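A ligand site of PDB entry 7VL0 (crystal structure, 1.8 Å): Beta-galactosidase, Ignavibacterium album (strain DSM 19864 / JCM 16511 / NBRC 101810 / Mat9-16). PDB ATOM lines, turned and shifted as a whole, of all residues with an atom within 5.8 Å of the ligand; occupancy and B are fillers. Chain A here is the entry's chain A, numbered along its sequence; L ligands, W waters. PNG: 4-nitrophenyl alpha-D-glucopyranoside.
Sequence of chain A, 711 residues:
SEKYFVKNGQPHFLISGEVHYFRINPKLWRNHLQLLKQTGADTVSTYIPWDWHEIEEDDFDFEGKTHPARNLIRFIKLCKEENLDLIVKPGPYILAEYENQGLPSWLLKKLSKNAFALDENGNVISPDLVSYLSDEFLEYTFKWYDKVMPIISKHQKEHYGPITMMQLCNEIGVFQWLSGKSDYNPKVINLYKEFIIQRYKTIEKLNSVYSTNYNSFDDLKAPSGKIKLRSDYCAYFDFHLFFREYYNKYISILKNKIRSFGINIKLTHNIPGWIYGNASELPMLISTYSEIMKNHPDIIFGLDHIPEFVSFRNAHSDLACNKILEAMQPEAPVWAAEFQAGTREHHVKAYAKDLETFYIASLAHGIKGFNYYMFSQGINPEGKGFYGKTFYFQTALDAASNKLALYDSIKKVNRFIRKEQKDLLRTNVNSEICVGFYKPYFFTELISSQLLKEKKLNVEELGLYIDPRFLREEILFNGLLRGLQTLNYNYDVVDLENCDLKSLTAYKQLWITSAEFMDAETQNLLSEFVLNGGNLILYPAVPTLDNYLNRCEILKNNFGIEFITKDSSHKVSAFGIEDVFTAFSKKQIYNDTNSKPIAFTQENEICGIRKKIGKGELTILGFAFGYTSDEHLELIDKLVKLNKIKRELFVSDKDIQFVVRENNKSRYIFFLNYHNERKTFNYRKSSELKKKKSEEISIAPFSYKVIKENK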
ATOM      1  N   LEU A  95      17.384 -12.715   0.601  1.00  0.00           N
ATOM      2  CA  LEU A  95      18.223 -13.908   0.937  1.00  0.00           C
ATOM      3  C   LEU A  95      18.543 -13.814   2.426  1.00  0.00           C
ATOM      4  O   LEU A  95      17.635 -14.055   3.223  1.00  0.00           O
ATOM      5  CB  LEU A  95      19.487 -13.860   0.055  1.00  0.00           C
ATOM      6  CG  LEU A  95      20.236 -15.157  -0.264  1.00  0.00           C
ATOM      7  CD1 LEU A  95      20.949 -14.973  -1.606  1.00  0.00           C
ATOM      8  CD2 LEU A  95      21.283 -15.516   0.805  1.00  0.00           C
ATOM      9  N   GLN A 101      13.550 -16.355   2.264  1.00  0.00           N
ATOM     10  CA  GLN A 101      14.471 -15.412   1.570  1.00  0.00           C
ATOM     11  C   GLN A 101      13.948 -13.967   1.635  1.00  0.00           C
ATOM     12  O   GLN A 101      14.313 -13.152   0.763  1.00  0.00           O
ATOM     13  CB  GLN A 101      14.684 -15.862   0.130  1.00  0.00           C
ATOM     14  CG  GLN A 101      14.899 -17.374  -0.015  1.00  0.00           C
ATOM     15  CD  GLN A 101      16.232 -17.848   0.505  1.00  0.00           C
ATOM     16  OE1 GLN A 101      17.070 -17.060   0.924  1.00  0.00           O
ATOM     17  NE2 GLN A 101      16.464 -19.143   0.438  1.00  0.00           N
ATOM     18  N   ASN A 170      18.048  -8.798  -4.825  1.00  0.00           N
ATOM     19  CA  ASN A 170      19.267  -9.439  -4.267  1.00  0.00           C
ATOM     20  C   ASN A 170      19.702 -10.549  -5.210  1.00  0.00           C
ATOM     21  O   ASN A 170      18.916 -11.495  -5.392  1.00  0.00           O
ATOM     22  CB  ASN A 170      19.017  -9.947  -2.852  1.00  0.00           C
ATOM     23  CG  ASN A 170      20.318 -10.308  -2.175  1.00  0.00           C
ATOM     24  OD1 ASN A 170      21.001  -9.419  -1.635  1.00  0.00           O
ATOM     25  ND2 ASN A 170      20.664 -11.581  -2.260  1.00  0.00           N
ATOM     26  N   GLU A 171      20.880 -10.417  -5.812  1.00  0.00           N
ATOM     27  CA  GLU A 171      21.542 -11.500  -6.594  1.00  0.00           C
ATOM     28  C   GLU A 171      20.565 -12.119  -7.595  1.00  0.00           C
ATOM     29  O   GLU A 171      20.225 -13.303  -7.477  1.00  0.00           O
ATOM     30  CB  GLU A 171      22.111 -12.559  -5.660  1.00  0.00           C
ATOM     31  CG  GLU A 171      23.197 -12.042  -4.735  1.00  0.00           C
ATOM     32  CD  GLU A 171      23.854 -13.091  -3.861  1.00  0.00           C
ATOM     33  OE1 GLU A 171      23.183 -14.115  -3.609  1.00  0.00           O
ATOM     34  OE2 GLU A 171      25.079 -12.904  -3.481  1.00  0.00           O
ATOM     35  N   VAL A 174      20.117 -15.998  -8.587  1.00  0.00           N
ATOM     36  CA  VAL A 174      20.931 -16.883  -7.689  1.00  0.00           C
ATOM     37  C   VAL A 174      20.077 -18.066  -7.233  1.00  0.00           C
ATOM     38  O   VAL A 174      20.578 -19.200  -7.267  1.00  0.00           O
ATOM     39  CB  VAL A 174      21.534 -16.138  -6.483  1.00  0.00           C
ATOM     40  CG1 VAL A 174      20.496 -15.761  -5.437  1.00  0.00           C
ATOM     41  CG2 VAL A 174      22.652 -16.940  -5.829  1.00  0.00           C
ATOM     42  N   PHE A 175      18.839 -17.791  -6.796  1.00  0.00           N
ATOM     43  CA  PHE A 175      17.853 -18.814  -6.355  1.00  0.00           C
ATOM     44  C   PHE A 175      17.702 -19.811  -7.495  1.00  0.00           C
ATOM     45  O   PHE A 175      17.883 -20.994  -7.255  1.00  0.00           O
ATOM     46  CB  PHE A 175      16.530 -18.193  -5.884  1.00  0.00           C
ATOM     47  CG  PHE A 175      16.664 -17.193  -4.772  1.00  0.00           C
ATOM     48  CD1 PHE A 175      17.001 -17.595  -3.492  1.00  0.00           C
ATOM     49  CD2 PHE A 175      16.501 -15.835  -5.004  1.00  0.00           C
ATOM     50  CE1 PHE A 175      17.206 -16.669  -2.475  1.00  0.00           C
ATOM     51  CE2 PHE A 175      16.706 -14.909  -3.987  1.00  0.00           C
ATOM     52  CZ  PHE A 175      17.052 -15.329  -2.722  1.00  0.00           C
ATOM     53  N   TRP A 177      19.834 -20.472 -10.063  1.00  0.00           N
ATOM     54  CA  TRP A 177      21.151 -21.138 -10.202  1.00  0.00           C
ATOM     55  C   TRP A 177      21.280 -22.287  -9.181  1.00  0.00           C
ATOM     56  O   TRP A 177      21.540 -23.405  -9.616  1.00  0.00           O
ATOM     57  CB  TRP A 177      22.271 -20.076 -10.074  1.00  0.00           C
ATOM     58  CG  TRP A 177      23.670 -20.598  -9.918  1.00  0.00           C
ATOM     59  CD1 TRP A 177      24.381 -21.379 -10.791  1.00  0.00           C
ATOM     60  CD2 TRP A 177      24.577 -20.270  -8.853  1.00  0.00           C
ATOM     61  NE1 TRP A 177      25.645 -21.609 -10.295  1.00  0.00           N
ATOM     62  CE2 TRP A 177      25.801 -20.932  -9.122  1.00  0.00           C
ATOM     63  CE3 TRP A 177      24.465 -19.509  -7.690  1.00  0.00           C
ATOM     64  CZ2 TRP A 177      26.897 -20.852  -8.264  1.00  0.00           C
ATOM     65  CZ3 TRP A 177      25.567 -19.393  -6.867  1.00  0.00           C
ATOM     66  CH2 TRP A 177      26.759 -20.070  -7.143  1.00  0.00           C
ATOM     67  N   LEU A 178      21.140 -22.031  -7.872  1.00  0.00           N
ATOM     68  CA  LEU A 178      21.328 -23.054  -6.789  1.00  0.00           C
ATOM     69  C   LEU A 178      20.237 -24.138  -6.833  1.00  0.00           C
ATOM     70  O   LEU A 178      20.527 -25.294  -6.448  1.00  0.00           O
ATOM     71  CB  LEU A 178      21.360 -22.351  -5.434  1.00  0.00           C
ATOM     72  CG  LEU A 178      22.565 -21.440  -5.176  1.00  0.00           C
ATOM     73  CD1 LEU A 178      22.576 -20.982  -3.737  1.00  0.00           C
ATOM     74  CD2 LEU A 178      23.881 -22.147  -5.456  1.00  0.00           C
ATOM     75  N   ILE A 271      26.559  -9.331  -7.051  1.00  0.00           N
ATOM     76  CA  ILE A 271      26.885 -10.473  -7.934  1.00  0.00           C
ATOM     77  C   ILE A 271      27.187 -11.701  -7.090  1.00  0.00           C
ATOM     78  O   ILE A 271      28.163 -11.687  -6.320  1.00  0.00           O
ATOM     79  CB  ILE A 271      28.081 -10.136  -8.833  1.00  0.00           C
ATOM     80  CG1 ILE A 271      27.842  -8.856  -9.643  1.00  0.00           C
ATOM     81  CG2 ILE A 271      28.398 -11.338  -9.694  1.00  0.00           C
ATOM     82  CD1 ILE A 271      29.114  -8.184 -10.076  1.00  0.00           C
ATOM     83  N   PRO A 272      26.382 -12.768  -7.244  1.00  0.00           N
ATOM     84  CA  PRO A 272      26.656 -14.050  -6.583  1.00  0.00           C
ATOM     85  C   PRO A 272      27.681 -14.860  -7.398  1.00  0.00           C
ATOM     86  O   PRO A 272      28.007 -14.444  -8.540  1.00  0.00           O
ATOM     87  CB  PRO A 272      25.287 -14.713  -6.586  1.00  0.00           C
ATOM     88  CG  PRO A 272      24.773 -14.326  -7.965  1.00  0.00           C
ATOM     89  CD  PRO A 272      25.204 -12.876  -8.127  1.00  0.00           C
ATOM     90  N   GLY A 273      28.181 -15.965  -6.815  1.00  0.00           N
ATOM     91  CA  GLY A 273      29.000 -16.931  -7.567  1.00  0.00           C
ATOM     92  C   GLY A 273      29.995 -17.707  -6.732  1.00  0.00           C
ATOM     93  O   GLY A 273      30.505 -18.760  -7.218  1.00  0.00           O
ATOM     94  N   TRP A 274      30.411 -17.215  -5.584  1.00  0.00           N
ATOM     95  CA  TRP A 274      31.332 -18.016  -4.739  1.00  0.00           C
ATOM     96  C   TRP A 274      30.563 -19.184  -4.123  1.00  0.00           C
ATOM     97  O   TRP A 274      29.400 -19.017  -3.711  1.00  0.00           O
ATOM     98  CB  TRP A 274      31.977 -17.170  -3.647  1.00  0.00           C
ATOM     99  CG  TRP A 274      33.004 -16.183  -4.068  1.00  0.00           C
ATOM    100  CD1 TRP A 274      32.774 -14.950  -4.603  1.00  0.00           C
ATOM    101  CD2 TRP A 274      34.429 -16.242  -3.817  1.00  0.00           C
ATOM    102  NE1 TRP A 274      33.927 -14.254  -4.727  1.00  0.00           N
ATOM    103  CE2 TRP A 274      34.964 -15.012  -4.247  1.00  0.00           C
ATOM    104  CE3 TRP A 274      35.290 -17.239  -3.325  1.00  0.00           C
ATOM    105  CZ2 TRP A 274      36.328 -14.729  -4.176  1.00  0.00           C
ATOM    106  CZ3 TRP A 274      36.634 -16.944  -3.239  1.00  0.00           C
ATOM    107  CH2 TRP A 274      37.145 -15.694  -3.640  1.00  0.00           C
ATOM    108  N   ILE A 275      31.211 -20.340  -4.042  1.00  0.00           N
ATOM    109  CA  ILE A 275      30.630 -21.520  -3.356  1.00  0.00           C
ATOM    110  C   ILE A 275      31.808 -22.398  -2.946  1.00  0.00           C
ATOM    111  O   ILE A 275      32.722 -22.563  -3.731  1.00  0.00           O
ATOM    112  CB  ILE A 275      29.560 -22.230  -4.198  1.00  0.00           C
ATOM    113  CG1 ILE A 275      28.715 -23.154  -3.309  1.00  0.00           C
ATOM    114  CG2 ILE A 275      30.149 -22.928  -5.427  1.00  0.00           C
ATOM    115  CD1 ILE A 275      27.539 -23.796  -4.019  1.00  0.00           C
ATOM    116  N   TYR A 276      31.804 -22.807  -1.682  1.00  0.00           N
ATOM    117  CA  TYR A 276      32.864 -23.657  -1.097  1.00  0.00           C
ATOM    118  C   TYR A 276      34.214 -22.945  -1.185  1.00  0.00           C
ATOM    119  O   TYR A 276      35.265 -23.619  -1.194  1.00  0.00           O
ATOM    120  CB  TYR A 276      32.877 -25.030  -1.765  1.00  0.00           C
ATOM    121  CG  TYR A 276      31.526 -25.672  -1.881  1.00  0.00           C
ATOM    122  CD1 TYR A 276      30.656 -25.758  -0.795  1.00  0.00           C
ATOM    123  CD2 TYR A 276      31.118 -26.235  -3.079  1.00  0.00           C
ATOM    124  CE1 TYR A 276      29.405 -26.351  -0.929  1.00  0.00           C
ATOM    125  CE2 TYR A 276      29.874 -26.858  -3.221  1.00  0.00           C
ATOM    126  CZ  TYR A 276      29.006 -26.899  -2.141  1.00  0.00           C
ATOM    127  OH  TYR A 276      27.772 -27.482  -2.340  1.00  0.00           O
ATOM    128  N   ASP A 304      29.946 -10.143  -4.374  1.00  0.00           N
ATOM    129  CA  ASP A 304      29.688 -10.840  -3.088  1.00  0.00           C
ATOM    130  C   ASP A 304      30.817 -11.858  -2.875  1.00  0.00           C
ATOM    131  O   ASP A 304      30.701 -12.965  -3.373  1.00  0.00           O
ATOM    132  CB  ASP A 304      28.272 -11.404  -3.088  1.00  0.00           C
ATOM    133  CG  ASP A 304      27.241 -10.286  -3.191  1.00  0.00           C
ATOM    134  OD1 ASP A 304      27.625  -9.088  -2.992  1.00  0.00           O
ATOM    135  OD2 ASP A 304      26.027 -10.615  -3.402  1.00  0.00           O
ATOM    136  N   ILE A 306      32.951 -14.467  -0.955  1.00  0.00           N
ATOM    137  CA  ILE A 306      32.920 -15.473   0.143  1.00  0.00           C
ATOM    138  C   ILE A 306      34.062 -16.465  -0.005  1.00  0.00           C
ATOM    139  O   ILE A 306      33.873 -17.633  -0.303  1.00  0.00           O
ATOM    140  CB  ILE A 306      31.593 -16.218   0.223  1.00  0.00           C
ATOM    141  CG1 ILE A 306      30.400 -15.296  -0.016  1.00  0.00           C
ATOM    142  CG2 ILE A 306      31.495 -16.951   1.560  1.00  0.00           C
ATOM    143  CD1 ILE A 306      29.119 -16.057  -0.178  1.00  0.00           C
ATOM    144  N   GLU A 338      29.249  -7.285  -0.699  1.00  0.00           N
ATOM    145  CA  GLU A 338      29.264  -8.203   0.448  1.00  0.00           C
ATOM    146  C   GLU A 338      30.706  -8.737   0.525  1.00  0.00           C
ATOM    147  O   GLU A 338      31.176  -9.398  -0.431  1.00  0.00           O
ATOM    148  CB  GLU A 338      28.247  -9.337   0.252  1.00  0.00           C
ATOM    149  CG  GLU A 338      26.794  -8.875   0.189  1.00  0.00           C
ATOM    150  CD  GLU A 338      25.822 -10.009  -0.022  1.00  0.00           C
ATOM    151  OE1 GLU A 338      26.209 -11.194   0.253  1.00  0.00           O
ATOM    152  OE2 GLU A 338      24.706  -9.742  -0.517  1.00  0.00           O
ATOM    153  N   ARG A 344      28.677 -17.320   7.522  1.00  0.00           N
ATOM    154  CA  ARG A 344      27.208 -17.564   7.448  1.00  0.00           C
ATOM    155  C   ARG A 344      26.828 -18.944   8.026  1.00  0.00           C
ATOM    156  O   ARG A 344      25.606 -19.177   8.233  1.00  0.00           O
ATOM    157  CB  ARG A 344      26.773 -17.480   5.993  1.00  0.00           C
ATOM    158  CG  ARG A 344      27.477 -18.509   5.118  1.00  0.00           C
ATOM    159  CD  ARG A 344      27.031 -18.353   3.671  1.00  0.00           C
ATOM    160  NE  ARG A 344      27.788 -19.246   2.787  1.00  0.00           N
ATOM    161  CZ  ARG A 344      27.504 -19.416   1.516  1.00  0.00           C
ATOM    162  NH1 ARG A 344      28.198 -20.252   0.756  1.00  0.00           N
ATOM    163  NH2 ARG A 344      26.542 -18.687   0.991  1.00  0.00           N
ATOM    164  N   PHE A 386      16.525 -18.773   8.717  1.00  0.00           N
ATOM    165  CA  PHE A 386      16.245 -19.835   7.716  1.00  0.00           C
ATOM    166  C   PHE A 386      16.739 -21.176   8.276  1.00  0.00           C
ATOM    167  O   PHE A 386      16.008 -22.164   8.163  1.00  0.00           O
ATOM    168  CB  PHE A 386      16.860 -19.498   6.358  1.00  0.00           C
ATOM    169  CG  PHE A 386      16.292 -20.295   5.214  1.00  0.00           C
ATOM    170  CD1 PHE A 386      16.666 -21.618   5.007  1.00  0.00           C
ATOM    171  CD2 PHE A 386      15.394 -19.726   4.317  1.00  0.00           C
ATOM    172  CE1 PHE A 386      16.133 -22.368   3.968  1.00  0.00           C
ATOM    173  CE2 PHE A 386      14.861 -20.475   3.263  1.00  0.00           C
ATOM    174  CZ  PHE A 386      15.232 -21.790   3.099  1.00  0.00           C
ATOM    175  N   TYR A 387      17.923 -21.181   8.897  1.00  0.00           N
ATOM    176  CA  TYR A 387      18.724 -22.392   9.220  1.00  0.00           C
ATOM    177  C   TYR A 387      19.028 -22.527  10.736  1.00  0.00           C
ATOM    178  O   TYR A 387      19.780 -23.452  11.084  1.00  0.00           O
ATOM    179  CB  TYR A 387      20.068 -22.354   8.484  1.00  0.00           C
ATOM    180  CG  TYR A 387      19.963 -22.389   6.980  1.00  0.00           C
ATOM    181  CD1 TYR A 387      19.576 -23.532   6.308  1.00  0.00           C
ATOM    182  CD2 TYR A 387      20.296 -21.270   6.225  1.00  0.00           C
ATOM    183  CE1 TYR A 387      19.492 -23.571   4.917  1.00  0.00           C
ATOM    184  CE2 TYR A 387      20.251 -21.291   4.832  1.00  0.00           C
ATOM    185  CZ  TYR A 387      19.839 -22.446   4.189  1.00  0.00           C
ATOM    186  OH  TYR A 387      19.776 -22.444   2.833  1.00  0.00           O
HETATM  187  C1  PNG L   1      24.359 -17.511  -1.290  1.00  0.00           C
HETATM  188  C2  PNG L   1      25.122 -16.222  -1.544  1.00  0.00           C
HETATM  189  C3  PNG L   1      25.763 -16.270  -2.934  1.00  0.00           C
HETATM  190  C4  PNG L   1      26.600 -17.553  -3.023  1.00  0.00           C
HETATM  191  C5  PNG L   1      25.710 -18.747  -2.835  1.00  0.00           C
HETATM  192  C6  PNG L   1      26.480 -20.085  -2.894  1.00  0.00           C
HETATM  193  C7  PNG L   1      22.174 -18.316  -1.900  1.00  0.00           C
HETATM  194  C8  PNG L   1      22.191 -19.317  -0.938  1.00  0.00           C
HETATM  195  C9  PNG L   1      21.078 -20.107  -0.725  1.00  0.00           C
HETATM  196  C10 PNG L   1      19.946 -19.875  -1.466  1.00  0.00           C
HETATM  197  C11 PNG L   1      19.900 -18.877  -2.413  1.00  0.00           C
HETATM  198  C12 PNG L   1      21.033 -18.099  -2.656  1.00  0.00           C
HETATM  199  N1  PNG L   1      18.836 -20.687  -1.246  1.00  0.00           N
HETATM  200  O1  PNG L   1      23.243 -17.535  -2.140  1.00  0.00           O
HETATM  201  O2  PNG L   1      24.283 -15.063  -1.413  1.00  0.00           O
HETATM  202  O3  PNG L   1      26.536 -15.098  -3.175  1.00  0.00           O
HETATM  203  O4  PNG L   1      27.235 -17.629  -4.307  1.00  0.00           O
HETATM  204  O5  PNG L   1      25.114 -18.719  -1.539  1.00  0.00           O
HETATM  205  O6  PNG L   1      27.558 -19.959  -1.964  1.00  0.00           O
HETATM  206  O7  PNG L   1      18.873 -21.468  -0.311  1.00  0.00           O
HETATM  207  O8  PNG L   1      17.749 -20.640  -2.125  1.00  0.00           O
HETATM  208  O   HOH W   1      23.535 -12.051  -0.955  1.00  0.00           O
HETATM  209  O   HOH W   2      29.327 -15.260  -3.825  1.00  0.00           O
HETATM  210  O   HOH W   3      25.454 -13.781   0.745  1.00  0.00           O
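The side-chain carboxylate of Glu 171 lies close to the side-chain carboxylate of Asp 304 (2.5 Å). N of Leu 95 is in hydrogen-bond range of O of Gln 101 (3.1 Å).
Leu 95 touches the ligand (CD1 to C12, 3.3 Å). Val 174 touches the ligand. Phe 175 touches the ligand (CD1 to C11, 3.3 Å). Trp 177 touches the ligand (CZ3 to O4, 3.5 Å). CD1 of Leu 178 touches C7 of the ligand, 3.3 Å away. Pro 272 touches the ligand. Ile 275 touches the ligand. Of the 20 residues printed, 13 come within 4 Å of the ligand.
The guanidinium group of Arg 344 lies within hydrogen-bond range of an oxygen (O6) of the ligand, 2.8 Å away. The side-chain hydroxyl (OH) of Tyr 387 is in hydrogen-bond range of an oxygen (O7) of the ligand, 3.4 Å away. An oxygen (O8) of the ligand sits at hydrogen-bond distance from the side-chain amide nitrogen (NE2) of Gln 101 (3.2 Å). O of Trp 274 is in hydrogen-bond range of O4 of the ligand (2.6 Å). The backbone NH (N) of Trp 274 is in hydrogen-bond range of an oxygen (O4) of the ligand. OE1 of Glu 171 lies within hydrogen-bond range of O2 of the ligand, 2.6 Å away. The backbone NH (N) of Gly 273 sits at hydrogen-bond distance from an oxygen (O4) of the ligand, 3.2 Å away.
Water W3 lies within hydrogen-bond range of the side-chain carboxylate of Glu 338 (2.7 Å) and an oxygen (O2) of the ligand (2.8 Å). Water W2 lies within hydrogen-bond range of the backbone carbonyl oxygen of Asp 304, the backbone NH of Trp 274, an oxygen (O3) of the ligand and the backbone NH of Gly 273. Water W1 lies within hydrogen-bond range of OE2 of Glu 338, OE2 of Glu 171, O2 of the ligand and ND2 of Asn 170.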
